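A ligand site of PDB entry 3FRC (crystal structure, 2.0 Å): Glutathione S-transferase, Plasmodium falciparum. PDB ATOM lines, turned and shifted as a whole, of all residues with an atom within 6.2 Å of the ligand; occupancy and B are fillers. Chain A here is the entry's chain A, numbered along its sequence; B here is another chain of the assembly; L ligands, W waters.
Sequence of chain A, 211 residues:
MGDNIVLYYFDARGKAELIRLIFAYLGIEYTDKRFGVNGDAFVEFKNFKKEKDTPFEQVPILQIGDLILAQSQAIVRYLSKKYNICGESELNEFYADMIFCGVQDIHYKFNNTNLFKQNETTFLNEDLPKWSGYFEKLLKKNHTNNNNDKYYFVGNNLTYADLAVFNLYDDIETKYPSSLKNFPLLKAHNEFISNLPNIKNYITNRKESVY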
ATOM      1  N   TYR A   9      21.655 -35.037 -33.501  1.00  0.00           N
ATOM      2  CA  TYR A   9      22.537 -34.001 -32.975  1.00  0.00           C
ATOM      3  C   TYR A   9      23.721 -33.897 -33.901  1.00  0.00           C
ATOM      4  O   TYR A   9      23.834 -34.650 -34.862  1.00  0.00           O
ATOM      5  CB  TYR A   9      22.986 -34.324 -31.550  1.00  0.00           C
ATOM      6  CG  TYR A   9      23.586 -33.140 -30.807  1.00  0.00           C
ATOM      7  CD1 TYR A   9      22.808 -32.020 -30.500  1.00  0.00           C
ATOM      8  CD2 TYR A   9      24.928 -33.131 -30.425  1.00  0.00           C
ATOM      9  CE1 TYR A   9      23.346 -30.931 -29.831  1.00  0.00           C
ATOM     10  CE2 TYR A   9      25.477 -32.038 -29.750  1.00  0.00           C
ATOM     11  CZ  TYR A   9      24.682 -30.945 -29.456  1.00  0.00           C
ATOM     12  OH  TYR A   9      25.210 -29.859 -28.783  1.00  0.00           O
ATOM     13  N   PHE A  10      24.618 -32.961 -33.602  1.00  0.00           N
ATOM     14  CA  PHE A  10      25.891 -32.869 -34.302  1.00  0.00           C
ATOM     15  C   PHE A  10      26.797 -33.988 -33.855  1.00  0.00           C
ATOM     16  O   PHE A  10      26.507 -34.677 -32.869  1.00  0.00           O
ATOM     17  CB  PHE A  10      26.525 -31.494 -34.038  1.00  0.00           C
ATOM     18  CG  PHE A  10      25.757 -30.371 -34.650  1.00  0.00           C
ATOM     19  CD1 PHE A  10      24.816 -29.675 -33.909  1.00  0.00           C
ATOM     20  CD2 PHE A  10      25.947 -30.043 -35.985  1.00  0.00           C
ATOM     21  CE1 PHE A  10      24.084 -28.645 -34.480  1.00  0.00           C
ATOM     22  CE2 PHE A  10      25.205 -29.005 -36.574  1.00  0.00           C
ATOM     23  CZ  PHE A  10      24.283 -28.303 -35.809  1.00  0.00           C
ATOM     24  N   GLY A  14      28.428 -32.245 -26.534  1.00  0.00           N
ATOM     25  CA  GLY A  14      27.550 -31.085 -26.369  1.00  0.00           C
ATOM     26  C   GLY A  14      26.297 -31.339 -25.551  1.00  0.00           C
ATOM     27  O   GLY A  14      26.387 -31.889 -24.445  1.00  0.00           O
ATOM     28  N   LYS A  15      25.153 -30.965 -26.107  1.00  0.00           N
ATOM     29  CA  LYS A  15      23.888 -31.033 -25.392  1.00  0.00           C
ATOM     30  C   LYS A  15      23.165 -32.385 -25.542  1.00  0.00           C
ATOM     31  O   LYS A  15      22.074 -32.564 -25.001  1.00  0.00           O
ATOM     32  CB  LYS A  15      22.978 -29.863 -25.832  1.00  0.00           C
ATOM     33  CG  LYS A  15      23.346 -28.493 -25.212  1.00  0.00           C
ATOM     34  CD  LYS A  15      22.608 -28.267 -23.881  1.00  0.00           C
ATOM     35  CE  LYS A  15      23.294 -27.244 -22.968  1.00  0.00           C
ATOM     36  NZ  LYS A  15      23.271 -25.838 -23.494  1.00  0.00           N
ATOM     37  N   PHE A  45      22.165 -29.999 -41.385  1.00  0.00           N
ATOM     38  CA  PHE A  45      21.331 -29.341 -40.369  1.00  0.00           C
ATOM     39  C   PHE A  45      20.274 -28.411 -40.998  1.00  0.00           C
ATOM     40  O   PHE A  45      19.179 -28.263 -40.471  1.00  0.00           O
ATOM     41  CB  PHE A  45      22.207 -28.560 -39.376  1.00  0.00           C
ATOM     42  CG  PHE A  45      21.440 -27.933 -38.241  1.00  0.00           C
ATOM     43  CD1 PHE A  45      20.635 -28.701 -37.410  1.00  0.00           C
ATOM     44  CD2 PHE A  45      21.540 -26.559 -37.997  1.00  0.00           C
ATOM     45  CE1 PHE A  45      19.926 -28.117 -36.364  1.00  0.00           C
ATOM     46  CE2 PHE A  45      20.843 -25.971 -36.945  1.00  0.00           C
ATOM     47  CZ  PHE A  45      20.029 -26.762 -36.130  1.00  0.00           C
ATOM     48  N   LYS A  49      16.124 -29.231 -40.604  1.00  0.00           N
ATOM     49  CA  LYS A  49      15.156 -28.248 -40.122  1.00  0.00           C
ATOM     50  C   LYS A  49      13.953 -28.095 -41.058  1.00  0.00           C
ATOM     51  O   LYS A  49      12.820 -27.939 -40.594  1.00  0.00           O
ATOM     52  CB  LYS A  49      15.836 -26.900 -39.882  1.00  0.00           C
ATOM     53  CG  LYS A  49      16.744 -26.879 -38.653  1.00  0.00           C
ATOM     54  CD  LYS A  49      17.220 -25.473 -38.307  1.00  0.00           C
ATOM     55  CE  LYS A  49      18.305 -24.970 -39.255  1.00  0.00           C
ATOM     56  NZ  LYS A  49      18.729 -23.581 -38.912  1.00  0.00           N
ATOM     57  N   PHE A  56      12.037 -25.153 -31.880  1.00  0.00           N
ATOM     58  CA  PHE A  56      12.970 -24.037 -31.710  1.00  0.00           C
ATOM     59  C   PHE A  56      14.180 -24.071 -32.660  1.00  0.00           C
ATOM     60  O   PHE A  56      15.155 -23.352 -32.437  1.00  0.00           O
ATOM     61  CB  PHE A  56      13.454 -23.968 -30.256  1.00  0.00           C
ATOM     62  CG  PHE A  56      12.357 -24.085 -29.231  1.00  0.00           C
ATOM     63  CD1 PHE A  56      12.325 -25.172 -28.362  1.00  0.00           C
ATOM     64  CD2 PHE A  56      11.379 -23.106 -29.106  1.00  0.00           C
ATOM     65  CE1 PHE A  56      11.327 -25.277 -27.393  1.00  0.00           C
ATOM     66  CE2 PHE A  56      10.374 -23.203 -28.147  1.00  0.00           C
ATOM     67  CZ  PHE A  56      10.351 -24.298 -27.290  1.00  0.00           C
ATOM     68  N   GLU A  57      14.109 -24.897 -33.699  1.00  0.00           N
ATOM     69  CA  GLU A  57      15.203 -25.056 -34.681  1.00  0.00           C
ATOM     70  C   GLU A  57      16.546 -25.405 -34.025  1.00  0.00           C
ATOM     71  O   GLU A  57      17.616 -25.002 -34.511  1.00  0.00           O
ATOM     72  CB  GLU A  57      15.310 -23.827 -35.581  1.00  0.00           C
ATOM     73  CG  GLU A  57      14.065 -23.614 -36.425  1.00  0.00           C
ATOM     74  CD  GLU A  57      14.101 -22.335 -37.233  1.00  0.00           C
ATOM     75  OE1 GLU A  57      14.792 -21.374 -36.835  1.00  0.00           O
ATOM     76  OE2 GLU A  57      13.419 -22.291 -38.280  1.00  0.00           O
ATOM     77  N   GLN A  58      16.464 -26.150 -32.923  1.00  0.00           N
ATOM     78  CA  GLN A  58      17.636 -26.599 -32.187  1.00  0.00           C
ATOM     79  C   GLN A  58      17.665 -28.130 -32.170  1.00  0.00           C
ATOM     80  O   GLN A  58      16.622 -28.799 -32.322  1.00  0.00           O
ATOM     81  CB  GLN A  58      17.587 -26.120 -30.738  1.00  0.00           C
ATOM     82  CG  GLN A  58      17.681 -24.611 -30.508  1.00  0.00           C
ATOM     83  CD  GLN A  58      17.411 -24.227 -29.046  1.00  0.00           C
ATOM     84  OE1 GLN A  58      16.609 -24.867 -28.359  1.00  0.00           O
ATOM     85  NE2 GLN A  58      18.086 -23.176 -28.579  1.00  0.00           N
ATOM     86  N   VAL A  59      18.861 -28.666 -32.006  1.00  0.00           N
ATOM     87  CA  VAL A  59      19.066 -30.064 -31.617  1.00  0.00           C
ATOM     88  C   VAL A  59      19.706 -30.038 -30.234  1.00  0.00           C
ATOM     89  O   VAL A  59      20.283 -29.020 -29.846  1.00  0.00           O
ATOM     90  CB  VAL A  59      19.932 -30.838 -32.653  1.00  0.00           C
ATOM     91  CG1 VAL A  59      19.102 -31.181 -33.903  1.00  0.00           C
ATOM     92  CG2 VAL A  59      21.185 -30.056 -33.031  1.00  0.00           C
ATOM     93  N   PRO A  60      19.621 -31.143 -29.461  1.00  0.00           N
ATOM     94  CA  PRO A  60      19.086 -32.474 -29.806  1.00  0.00           C
ATOM     95  C   PRO A  60      17.586 -32.537 -30.063  1.00  0.00           C
ATOM     96  O   PRO A  60      16.801 -31.810 -29.444  1.00  0.00           O
ATOM     97  CB  PRO A  60      19.441 -33.315 -28.587  1.00  0.00           C
ATOM     98  CG  PRO A  60      19.505 -32.343 -27.466  1.00  0.00           C
ATOM     99  CD  PRO A  60      20.104 -31.107 -28.068  1.00  0.00           C
ATOM    100  N   ALA A  70      11.965 -32.101 -28.144  1.00  0.00           N
ATOM    101  CA  ALA A  70      13.085 -31.164 -28.113  1.00  0.00           C
ATOM    102  C   ALA A  70      13.426 -30.764 -26.681  1.00  0.00           C
ATOM    103  O   ALA A  70      12.678 -31.080 -25.741  1.00  0.00           O
ATOM    104  CB  ALA A  70      12.789 -29.934 -28.950  1.00  0.00           C
ATOM    105  N   GLN A  71      14.553 -30.057 -26.541  1.00  0.00           N
ATOM    106  CA  GLN A  71      15.079 -29.542 -25.259  1.00  0.00           C
ATOM    107  C   GLN A  71      15.656 -30.655 -24.404  1.00  0.00           C
ATOM    108  O   GLN A  71      14.916 -31.454 -23.815  1.00  0.00           O
ATOM    109  CB  GLN A  71      14.021 -28.716 -24.505  1.00  0.00           C
ATOM    110  CG  GLN A  71      13.725 -27.349 -25.135  1.00  0.00           C
ATOM    111  CD  GLN A  71      14.887 -26.377 -25.080  1.00  0.00           C
ATOM    112  OE1 GLN A  71      15.789 -26.526 -24.254  1.00  0.00           O
ATOM    113  NE2 GLN A  71      14.857 -25.353 -25.931  1.00  0.00           N
ATOM    114  N   SER A  72      16.983 -30.693 -24.341  1.00  0.00           N
ATOM    115  CA  SER A  72      17.735 -31.780 -23.708  1.00  0.00           C
ATOM    116  C   SER A  72      17.351 -32.057 -22.248  1.00  0.00           C
ATOM    117  O   SER A  72      17.241 -33.213 -21.854  1.00  0.00           O
ATOM    118  CB  SER A  72      19.236 -31.526 -23.813  1.00  0.00           C
ATOM    119  OG  SER A  72      19.618 -30.385 -23.065  1.00  0.00           O
ATOM    120  N   GLN A  73      17.153 -31.005 -21.452  1.00  0.00           N
ATOM    121  CA  GLN A  73      16.794 -31.211 -20.041  1.00  0.00           C
ATOM    122  C   GLN A  73      15.403 -31.818 -19.901  1.00  0.00           C
ATOM    123  O   GLN A  73      15.176 -32.643 -19.016  1.00  0.00           O
ATOM    124  CB  GLN A  73      16.788 -29.936 -19.218  1.00  0.00           C
ATOM    125  CG  GLN A  73      17.969 -29.020 -19.312  1.00  0.00           C
ATOM    126  CD  GLN A  73      17.552 -27.641 -18.829  1.00  0.00           C
ATOM    127  OE1 GLN A  73      17.753 -26.655 -19.521  1.00  0.00           O
ATOM    128  NE2 GLN A  73      16.908 -27.595 -17.648  1.00  0.00           N
ATOM    129  N   ASN A 111      31.332 -24.796 -20.952  1.00  0.00           N
ATOM    130  CA  ASN A 111      31.068 -24.664 -22.387  1.00  0.00           C
ATOM    131  C   ASN A 111      31.554 -23.349 -22.980  1.00  0.00           C
ATOM    132  O   ASN A 111      32.102 -23.322 -24.084  1.00  0.00           O
ATOM    133  CB  ASN A 111      29.577 -24.860 -22.706  1.00  0.00           C
ATOM    134  CG  ASN A 111      29.100 -26.288 -22.454  1.00  0.00           C
ATOM    135  OD1 ASN A 111      29.877 -27.239 -22.524  1.00  0.00           O
ATOM    136  ND2 ASN A 111      27.812 -26.437 -22.168  1.00  0.00           N
ATOM    137  N   LEU A 115      34.373 -24.424 -25.550  1.00  0.00           N
ATOM    138  CA  LEU A 115      33.894 -24.322 -26.928  1.00  0.00           C
ATOM    139  C   LEU A 115      33.942 -22.902 -27.459  1.00  0.00           C
ATOM    140  O   LEU A 115      34.392 -22.666 -28.575  1.00  0.00           O
ATOM    141  CB  LEU A 115      32.463 -24.868 -27.047  1.00  0.00           C
ATOM    142  CG  LEU A 115      32.183 -26.313 -26.616  1.00  0.00           C
ATOM    143  CD1 LEU A 115      30.690 -26.553 -26.536  1.00  0.00           C
ATOM    144  CD2 LEU A 115      32.848 -27.324 -27.566  1.00  0.00           C
ATOM    145  N   PHE A 116      33.499 -21.954 -26.631  1.00  0.00           N
ATOM    146  CA  PHE A 116      33.267 -20.597 -27.101  1.00  0.00           C
ATOM    147  C   PHE A 116      34.438 -19.653 -26.811  1.00  0.00           C
ATOM    148  O   PHE A 116      34.290 -18.436 -26.827  1.00  0.00           O
ATOM    149  CB  PHE A 116      31.908 -20.084 -26.590  1.00  0.00           C
ATOM    150  CG  PHE A 116      30.753 -21.044 -26.851  1.00  0.00           C
ATOM    151  CD1 PHE A 116      30.371 -21.373 -28.150  1.00  0.00           C
ATOM    152  CD2 PHE A 116      30.046 -21.610 -25.790  1.00  0.00           C
ATOM    153  CE1 PHE A 116      29.309 -22.260 -28.397  1.00  0.00           C
ATOM    154  CE2 PHE A 116      28.978 -22.498 -26.025  1.00  0.00           C
ATOM    155  CZ  PHE A 116      28.613 -22.821 -27.331  1.00  0.00           C
ATOM    156  N   CYS B 101      11.831 -24.843 -20.952  1.00  0.00           N
ATOM    157  CA  CYS B 101      13.245 -24.894 -21.321  1.00  0.00           C
ATOM    158  C   CYS B 101      13.568 -23.919 -22.468  1.00  0.00           C
ATOM    159  O   CYS B 101      14.627 -23.309 -22.475  1.00  0.00           O
ATOM    160  CB  CYS B 101      13.671 -26.323 -21.675  1.00  0.00           C
ATOM    161  SG  CYS B 101      13.781 -27.394 -20.239  1.00  0.00           S
ATOM    162  N   GLY B 102      12.633 -23.771 -23.410  1.00  0.00           N
ATOM    163  CA  GLY B 102      12.777 -22.825 -24.524  1.00  0.00           C
ATOM    164  C   GLY B 102      12.727 -21.385 -24.057  1.00  0.00           C
ATOM    165  O   GLY B 102      13.522 -20.547 -24.498  1.00  0.00           O
ATOM    166  N   ASP B 105      16.118 -20.452 -22.716  1.00  0.00           N
ATOM    167  CA  ASP B 105      17.108 -20.118 -23.740  1.00  0.00           C
ATOM    168  C   ASP B 105      17.041 -18.653 -24.120  1.00  0.00           C
ATOM    169  O   ASP B 105      18.059 -17.961 -24.132  1.00  0.00           O
ATOM    170  CB  ASP B 105      16.924 -20.961 -25.005  1.00  0.00           C
ATOM    171  CG  ASP B 105      17.404 -22.372 -24.815  1.00  0.00           C
ATOM    172  OD1 ASP B 105      18.140 -22.630 -23.846  1.00  0.00           O
ATOM    173  OD2 ASP B 105      17.046 -23.231 -25.636  1.00  0.00           O
ATOM    174  N   LYS B 130      12.786 -14.072 -33.738  1.00  0.00           N
ATOM    175  CA  LYS B 130      12.856 -15.484 -34.099  1.00  0.00           C
ATOM    176  C   LYS B 130      12.191 -16.373 -33.037  1.00  0.00           C
ATOM    177  O   LYS B 130      11.404 -17.262 -33.358  1.00  0.00           O
ATOM    178  CB  LYS B 130      14.322 -15.865 -34.269  1.00  0.00           C
ATOM    179  CG  LYS B 130      14.594 -17.262 -34.764  1.00  0.00           C
ATOM    180  CD  LYS B 130      16.077 -17.458 -34.992  1.00  0.00           C
ATOM    181  CE  LYS B 130      16.810 -17.706 -33.694  1.00  0.00           C
ATOM    182  NZ  LYS B 130      18.207 -18.143 -33.949  1.00  0.00           N
HETATM  183  N1  LIG L   1      18.374 -25.453 -24.557  1.00  0.00           N
HETATM  184  C1  LIG L   1      18.618 -26.310 -25.711  1.00  0.00           C
HETATM  185  C2  LIG L   1      18.745 -27.745 -25.292  1.00  0.00           C
HETATM  186  O1  LIG L   1      18.323 -28.647 -26.054  1.00  0.00           O
HETATM  187  C3  LIG L   1      19.903 -25.845 -26.373  1.00  0.00           C
HETATM  188  C4  LIG L   1      20.240 -26.649 -27.617  1.00  0.00           C
HETATM  189  C5  LIG L   1      21.235 -25.934 -28.496  1.00  0.00           C
HETATM  190  O2  LIG L   1      21.707 -24.846 -28.176  1.00  0.00           O
HETATM  191  O3  LIG L   1      19.284 -28.006 -24.192  1.00  0.00           O
HETATM  192  C6  LIG L   1      22.505 -26.033 -30.586  1.00  0.00           C
HETATM  193  C7  LIG L   1      21.731 -25.819 -31.845  1.00  0.00           C
HETATM  194  O4  LIG L   1      21.083 -26.734 -32.326  1.00  0.00           O
HETATM  195  N2  LIG L   1      21.566 -26.571 -29.609  1.00  0.00           N
HETATM  196  C8  LIG L   1      23.592 -27.080 -30.783  1.00  0.00           C
HETATM  197  S1  LIG L   1      24.886 -26.411 -31.800  1.00  0.00           S
HETATM  198 BR1  LIG L   1      27.175 -27.127 -25.346  1.00  0.00          BR
HETATM  199  C9  LIG L   1      25.991 -25.532 -29.557  1.00  0.00           C
HETATM  200  C10 LIG L   1      25.319 -25.031 -28.430  1.00  0.00           C
HETATM  201  C11 LIG L   1      25.667 -25.494 -27.156  1.00  0.00           C
HETATM  202  C12 LIG L   1      26.665 -26.455 -27.035  1.00  0.00           C
HETATM  203  C13 LIG L   1      27.325 -26.950 -28.160  1.00  0.00           C
HETATM  204  C14 LIG L   1      26.983 -26.495 -29.424  1.00  0.00           C
HETATM  205  C15 LIG L   1      25.631 -25.062 -30.945  1.00  0.00           C
HETATM  206  N3  LIG L   1      21.759 -24.606 -32.377  1.00  0.00           N
HETATM  207  C16 LIG L   1      21.069 -24.195 -33.592  1.00  0.00           C
HETATM  208  C17 LIG L   1      21.654 -22.922 -34.139  1.00  0.00           C
HETATM  209  O5  LIG L   1      22.616 -22.386 -33.551  1.00  0.00           O
HETATM  210  O6  LIG L   1      21.151 -22.437 -35.182  1.00  0.00           O
HETATM  211  O   HOH W   1      22.684 -21.920 -37.656  1.00  0.00           O
HETATM  212  O   HOH W   2      22.783 -22.224 -30.279  1.00  0.00           O
HETATM  213  O   HOH W   3      20.810 -25.054 -22.926  1.00  0.00           O
HETATM  214  O   HOH W   4      18.896 -23.155 -36.116  1.00  0.00           O
HETATM  215  O   HOH W   5      16.795 -28.182 -22.101  1.00  0.00           O
HETATM  216  O   HOH W   6      21.684 -22.954 -26.409  1.00  0.00           O
HETATM  217  O   HOH W   7      17.060 -24.335 -21.794  1.00  0.00           O
HETATM  218  O   HOH W   8      27.664 -29.611 -29.988  1.00  0.00           O
HETATM  219  O   HOH W   9      16.703 -29.321 -28.230  1.00  0.00           O
HETATM  220  O   HOH W  10      29.944 -29.159 -28.543  1.00  0.00           O
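The backbone NH (N) of Ser 72 is in hydrogen-bond range of an oxygen (O1) of the ligand (3.0 Å).
An oxygen (O3) of the ligand lies within hydrogen-bond range of the side-chain hydroxyl (OG) of Ser 72, at 2.7 Å.
An oxygen (O4) of the ligand lies within hydrogen-bond range of the backbone NH (N) of Val 59, 3.0 Å away.
O of Val 59 is in hydrogen-bond range of N2 of the ligand, 2.8 Å away.
The side-chain carboxylate (OD2) of Asp 105 of chain B is in salt-bridge range of a nitrogen (N1) of the ligand (2.8 Å).
The side-chain amide oxygen (OE1) of Gln 71 is in hydrogen-bond range of a nitrogen (N1) of the ligand (2.8 Å).
The side-chain amide nitrogen (NE2) of Gln 71 is in hydrogen-bond range of the side-chain carboxylate (OD2) of Asp 105 of chain B (3.1 Å).
The side-chain carboxylate (OD2) of Asp 105 of chain B sits at hydrogen-bond distance from the side-chain amide nitrogen (NE2) of Gln 58.
NE2 of Gln 71 is in hydrogen-bond range of OE1 of Gln 58 (3.0 Å).
The backbone carbonyl oxygen (O) of Asn 111 lies close to the backbone NH (N) of Phe 116.
The side-chain hydroxyl of Tyr 9 sits at hydrogen-bond distance from the backbone NH of Lys 15, 2.9 Å away.
Tyr 9 touches the ligand (OH to C13, 3.7 Å).
Phe 10 touches the ligand.
Lys 15 touches the ligand.
Phe 45 touches the ligand (CZ to C16, 3.8 Å).
Glu 57 touches the ligand (O to C16, 3.7 Å).
Gln 58 touches the ligand.
Pro 60 touches the ligand.
Asn 111 touches the ligand.
CD1 of Leu 115 touches BR1 of the ligand, at 3.8 Å.
Phe 116 touches the ligand.
Hydrophobic or aromatic side chains within 4 Å of the ligand: Tyr 9, Phe 10, Phe 45, Val 59, Pro 60, Leu 115 and Phe 116.
14 residues have an atom within 4 Å of the ligand: Tyr 9, Phe 10, Lys 15, Phe 45, Glu 57, Gln 58, Val 59, Pro 60, Gln 71, Ser 72, Asn 111, Leu 115, Phe 116 and Asp 105 of chain B.
Water W4 lies within hydrogen-bond range of O6 of the ligand (2.5 Å), O of Glu 57 (2.8 Å) and NZ of Lys 49 (2.8 Å).
Water W9 lies within hydrogen-bond range of the backbone carbonyl oxygen of Pro 60 (2.8 Å), an oxygen (O1) of the ligand (2.8 Å) and the backbone NH of Gln 71 (2.8 Å).
Water W3 bridges NZ of Lys 15 (2.6 Å) and N1 of the ligand (3.0 Å).
Water W5 lies within hydrogen-bond range of OE1 of Gln 71 (2.9 Å), N of Gln 73 (2.9 Å), O3 of the ligand (3.3 Å), N of Ser 72 (3.4 Å) and SG of Cys 101 of chain B (3.6 Å).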
